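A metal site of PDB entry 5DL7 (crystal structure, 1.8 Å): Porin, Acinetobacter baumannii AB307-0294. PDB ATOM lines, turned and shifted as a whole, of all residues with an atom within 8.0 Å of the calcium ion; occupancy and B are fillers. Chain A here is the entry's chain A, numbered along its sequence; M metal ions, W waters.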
ATOM      1  N   ASP A  33     -18.726 -24.490  -3.062  1.00  0.00           N
ATOM      2  CA  ASP A  33     -19.883 -25.246  -3.649  1.00  0.00           C
ATOM      3  C   ASP A  33     -20.567 -24.305  -4.613  1.00  0.00           C
ATOM      4  O   ASP A  33     -21.339 -23.434  -4.158  1.00  0.00           O
ATOM      5  CB  ASP A  33     -20.832 -25.552  -2.523  1.00  0.00           C
ATOM      6  CG  ASP A  33     -22.204 -26.259  -3.027  1.00  0.00           C
ATOM      7  OD1 ASP A  33     -22.059 -27.052  -4.012  1.00  0.00           O
ATOM      8  OD2 ASP A  33     -23.325 -25.958  -2.419  1.00  0.00           O
ATOM      9  N   ARG A  34     -20.493 -24.563  -5.910  1.00  0.00           N
ATOM     10  CA  ARG A  34     -21.254 -23.787  -6.877  1.00  0.00           C
ATOM     11  C   ARG A  34     -22.363 -24.832  -7.372  1.00  0.00           C
ATOM     12  O   ARG A  34     -22.134 -25.698  -8.156  1.00  0.00           O
ATOM     13  CB  ARG A  34     -20.374 -23.339  -7.998  1.00  0.00           C
ATOM     14  CG  ARG A  34     -21.088 -22.614  -9.144  1.00  0.00           C
ATOM     15  CD  ARG A  34     -20.224 -22.158 -10.240  1.00  0.00           C
ATOM     16  NE  ARG A  34     -19.365 -21.030  -9.764  1.00  0.00           N
ATOM     17  CZ  ARG A  34     -18.213 -20.667 -10.268  1.00  0.00           C
ATOM     18  NH1 ARG A  34     -17.741 -21.161 -11.382  1.00  0.00           N
ATOM     19  NH2 ARG A  34     -17.600 -19.545  -9.824  1.00  0.00           N
ATOM     20  N   ASP A  35     -23.536 -24.674  -6.811  1.00  0.00           N
ATOM     21  CA  ASP A  35     -24.620 -25.664  -7.036  1.00  0.00           C
ATOM     22  C   ASP A  35     -25.445 -25.142  -8.129  1.00  0.00           C
ATOM     23  O   ASP A  35     -26.305 -24.238  -8.017  1.00  0.00           O
ATOM     24  CB  ASP A  35     -25.394 -25.822  -5.776  1.00  0.00           C
ATOM     25  CG  ASP A  35     -26.430 -26.932  -5.916  1.00  0.00           C
ATOM     26  OD1 ASP A  35     -26.825 -27.252  -7.044  1.00  0.00           O
ATOM     27  OD2 ASP A  35     -26.788 -27.330  -4.774  1.00  0.00           O
ATOM     28  N   TYR A  36     -25.252 -25.765  -9.293  1.00  0.00           N
ATOM     29  CA  TYR A  36     -25.965 -25.398 -10.519  1.00  0.00           C
ATOM     30  C   TYR A  36     -27.423 -25.569 -10.383  1.00  0.00           C
ATOM     31  O   TYR A  36     -27.905 -26.629  -9.885  1.00  0.00           O
ATOM     32  CB  TYR A  36     -25.478 -26.237 -11.701  1.00  0.00           C
ATOM     33  CG  TYR A  36     -24.053 -26.251 -11.892  1.00  0.00           C
ATOM     34  CD1 TYR A  36     -23.313 -25.094 -12.115  1.00  0.00           C
ATOM     35  CD2 TYR A  36     -23.319 -27.499 -11.858  1.00  0.00           C
ATOM     36  CE1 TYR A  36     -21.927 -25.092 -12.372  1.00  0.00           C
ATOM     37  CE2 TYR A  36     -21.979 -27.536 -12.079  1.00  0.00           C
ATOM     38  CZ  TYR A  36     -21.246 -26.299 -12.319  1.00  0.00           C
ATOM     39  OH  TYR A  36     -19.926 -26.444 -12.546  1.00  0.00           O
ATOM     40  N   LYS A  37     -28.224 -24.604 -10.834  1.00  0.00           N
ATOM     41  CA  LYS A  37     -29.696 -24.709 -10.800  1.00  0.00           C
ATOM     42  C   LYS A  37     -30.257 -25.780 -11.727  1.00  0.00           C
ATOM     43  O   LYS A  37     -31.245 -26.429 -11.315  1.00  0.00           O
ATOM     44  CB  LYS A  37     -30.383 -23.376 -10.990  1.00  0.00           C
ATOM     45  CG  LYS A  37     -29.939 -22.506  -9.796  1.00  0.00           C
ATOM     46  CD  LYS A  37     -30.880 -21.430  -9.204  1.00  0.00           C
ATOM     47  CE  LYS A  37     -30.803 -20.073  -9.880  1.00  0.00           C
ATOM     48  NZ  LYS A  37     -32.267 -19.565  -9.764  1.00  0.00           N
ATOM     49  N   LYS A  38     -29.702 -25.955 -12.912  1.00  0.00           N
ATOM     50  CA  LYS A  38     -30.237 -26.815 -13.950  1.00  0.00           C
ATOM     51  C   LYS A  38     -29.362 -28.021 -14.213  1.00  0.00           C
ATOM     52  O   LYS A  38     -29.477 -28.597 -15.273  1.00  0.00           O
ATOM     53  CB  LYS A  38     -30.412 -26.009 -15.203  1.00  0.00           C
ATOM     54  CG  LYS A  38     -31.544 -24.947 -15.014  1.00  0.00           C
ATOM     55  CD  LYS A  38     -31.848 -24.246 -16.333  1.00  0.00           C
ATOM     56  CE  LYS A  38     -30.691 -23.298 -16.845  1.00  0.00           C
ATOM     57  NZ  LYS A  38     -30.471 -23.184 -18.392  1.00  0.00           N
ATOM     58  N   ASP A  39     -28.395 -28.359 -13.326  1.00  0.00           N
ATOM     59  CA  ASP A  39     -27.593 -29.634 -13.396  1.00  0.00           C
ATOM     60  C   ASP A  39     -27.176 -29.994 -14.813  1.00  0.00           C
ATOM     61  O   ASP A  39     -27.635 -31.010 -15.355  1.00  0.00           O
ATOM     62  CB  ASP A  39     -28.346 -30.807 -12.721  1.00  0.00           C
ATOM     63  CG  ASP A  39     -28.605 -30.516 -11.249  1.00  0.00           C
ATOM     64  OD1 ASP A  39     -27.969 -29.516 -10.700  1.00  0.00           O
ATOM     65  OD2 ASP A  39     -29.363 -31.334 -10.645  1.00  0.00           O
ATOM     66  N   PRO A  40     -26.248 -29.203 -15.389  1.00  0.00           N
ATOM     67  CA  PRO A  40     -25.931 -29.378 -16.789  1.00  0.00           C
ATOM     68  C   PRO A  40     -25.150 -30.680 -16.754  1.00  0.00           C
ATOM     69  O   PRO A  40     -24.046 -30.788 -16.181  1.00  0.00           O
ATOM     70  CB  PRO A  40     -25.064 -28.142 -17.133  1.00  0.00           C
ATOM     71  CG  PRO A  40     -24.448 -27.718 -15.781  1.00  0.00           C
ATOM     72  CD  PRO A  40     -25.486 -28.074 -14.774  1.00  0.00           C
ATOM     73  N   TYR A  43     -23.106 -33.104 -13.992  1.00  0.00           N
ATOM     74  CA  TYR A  43     -22.705 -32.639 -12.684  1.00  0.00           C
ATOM     75  C   TYR A  43     -23.836 -31.834 -12.059  1.00  0.00           C
ATOM     76  O   TYR A  43     -24.527 -31.095 -12.793  1.00  0.00           O
ATOM     77  CB  TYR A  43     -21.450 -31.708 -12.781  1.00  0.00           C
ATOM     78  CG  TYR A  43     -20.214 -32.486 -13.183  1.00  0.00           C
ATOM     79  CD1 TYR A  43     -19.866 -33.607 -12.482  1.00  0.00           C
ATOM     80  CD2 TYR A  43     -19.481 -32.144 -14.316  1.00  0.00           C
ATOM     81  CE1 TYR A  43     -18.814 -34.404 -12.895  1.00  0.00           C
ATOM     82  CE2 TYR A  43     -18.405 -32.914 -14.751  1.00  0.00           C
ATOM     83  CZ  TYR A  43     -18.087 -34.037 -14.016  1.00  0.00           C
ATOM     84  OH  TYR A  43     -17.087 -34.881 -14.408  1.00  0.00           O
ATOM     85  N   THR A  44     -24.054 -32.036 -10.750  1.00  0.00           N
ATOM     86  CA  THR A  44     -25.014 -31.235 -10.014  1.00  0.00           C
ATOM     87  C   THR A  44     -24.481 -29.963  -9.411  1.00  0.00           C
ATOM     88  O   THR A  44     -25.286 -29.069  -9.064  1.00  0.00           O
ATOM     89  CB  THR A  44     -25.700 -31.974  -8.945  1.00  0.00           C
ATOM     90  OG1 THR A  44     -26.899 -31.153  -8.590  1.00  0.00           O
ATOM     91  CG2 THR A  44     -24.839 -32.313  -7.855  1.00  0.00           C
ATOM     92  N   ALA A  45     -23.164 -29.906  -9.319  1.00  0.00           N
ATOM     93  CA  ALA A  45     -22.473 -28.788  -8.639  1.00  0.00           C
ATOM     94  C   ALA A  45     -20.986 -28.923  -8.928  1.00  0.00           C
ATOM     95  O   ALA A  45     -20.533 -30.020  -9.343  1.00  0.00           O
ATOM     96  CB  ALA A  45     -22.714 -28.834  -7.121  1.00  0.00           C
ATOM     97  N   ALA A  46     -20.264 -27.792  -8.858  1.00  0.00           N
ATOM     98  CA  ALA A  46     -18.785 -27.764  -8.769  1.00  0.00           C
ATOM     99  C   ALA A  46     -18.497 -27.679  -7.288  1.00  0.00           C
ATOM    100  O   ALA A  46     -19.015 -26.742  -6.610  1.00  0.00           O
ATOM    101  CB  ALA A  46     -18.176 -26.582  -9.471  1.00  0.00           C
ATOM    102  N   ARG A  47     -17.674 -28.581  -6.724  1.00  0.00           N
ATOM    103  CA  ARG A  47     -17.590 -28.622  -5.260  1.00  0.00           C
ATOM    104  C   ARG A  47     -16.270 -29.231  -4.857  1.00  0.00           C
ATOM    105  O   ARG A  47     -15.814 -30.160  -5.518  1.00  0.00           O
ATOM    106  CB  ARG A  47     -18.662 -29.516  -4.652  1.00  0.00           C
ATOM    107  CG  ARG A  47     -18.880 -29.512  -3.157  1.00  0.00           C
ATOM    108  CD  ARG A  47     -20.095 -30.386  -2.724  1.00  0.00           C
ATOM    109  NE  ARG A  47     -21.281 -29.752  -3.186  1.00  0.00           N
ATOM    110  CZ  ARG A  47     -22.561 -30.234  -3.085  1.00  0.00           C
ATOM    111  NH1 ARG A  47     -22.751 -31.430  -2.636  1.00  0.00           N
ATOM    112  NH2 ARG A  47     -23.576 -29.560  -3.556  1.00  0.00           N
ATOM    113  N   TYR A  88     -18.311 -34.370  -8.566  1.00  0.00           N
ATOM    114  CA  TYR A  88     -18.675 -32.998  -8.780  1.00  0.00           C
ATOM    115  C   TYR A  88     -17.786 -32.358  -9.794  1.00  0.00           C
ATOM    116  O   TYR A  88     -16.621 -32.718  -9.983  1.00  0.00           O
ATOM    117  CB  TYR A  88     -18.591 -32.259  -7.417  1.00  0.00           C
ATOM    118  CG  TYR A  88     -19.539 -32.740  -6.409  1.00  0.00           C
ATOM    119  CD1 TYR A  88     -20.861 -32.528  -6.550  1.00  0.00           C
ATOM    120  CD2 TYR A  88     -19.148 -33.558  -5.389  1.00  0.00           C
ATOM    121  CE1 TYR A  88     -21.755 -33.036  -5.605  1.00  0.00           C
ATOM    122  CE2 TYR A  88     -19.982 -34.128  -4.513  1.00  0.00           C
ATOM    123  CZ  TYR A  88     -21.302 -33.879  -4.616  1.00  0.00           C
ATOM    124  OH  TYR A  88     -22.145 -34.437  -3.721  1.00  0.00           O
ATOM    125  N   SER A 405     -26.409 -20.654 -14.186  1.00  0.00           N
ATOM    126  CA  SER A 405     -27.257 -20.278 -12.998  1.00  0.00           C
ATOM    127  C   SER A 405     -26.846 -21.206 -11.866  1.00  0.00           C
ATOM    128  O   SER A 405     -26.782 -22.453 -12.092  1.00  0.00           O
ATOM    129  CB  SER A 405     -28.782 -20.382 -13.327  1.00  0.00           C
ATOM    130  OG  SER A 405     -29.081 -19.505 -14.398  1.00  0.00           O
ATOM    131  N   ALA A 406     -26.640 -20.652 -10.669  1.00  0.00           N
ATOM    132  CA  ALA A 406     -26.122 -21.413  -9.568  1.00  0.00           C
ATOM    133  C   ALA A 406     -26.395 -20.702  -8.282  1.00  0.00           C
ATOM    134  O   ALA A 406     -26.487 -19.458  -8.223  1.00  0.00           O
ATOM    135  CB  ALA A 406     -24.628 -21.671  -9.757  1.00  0.00           C
ATOM    136  N   ASN A 407     -26.412 -21.438  -7.216  1.00  0.00           N
ATOM    137  CA  ASN A 407     -26.313 -20.891  -5.884  1.00  0.00           C
ATOM    138  C   ASN A 407     -24.939 -21.349  -5.320  1.00  0.00           C
ATOM    139  O   ASN A 407     -24.632 -22.560  -5.209  1.00  0.00           O
ATOM    140  CB  ASN A 407     -27.391 -21.467  -4.995  1.00  0.00           C
ATOM    141  CG  ASN A 407     -28.774 -20.980  -5.382  1.00  0.00           C
ATOM    142  OD1 ASN A 407     -28.986 -19.885  -5.759  1.00  0.00           O
ATOM    143  ND2 ASN A 407     -29.692 -21.799  -5.222  1.00  0.00           N
HETATM  144 CA    CA M   1     -27.604 -28.616  -8.605  1.00  0.00          CA
HETATM  145  O   HOH W   1     -29.480 -27.764  -7.623  1.00  0.00           O
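N of Asp 35 sits at hydrogen-bond distance from O of Asn 407 (2.9 Å).
The calcium ion is bound by OD1 of Asp 35, water W1, OD1 of Asp 39, O of Tyr 36, O of Thr 44 and OG1 of Thr 44.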
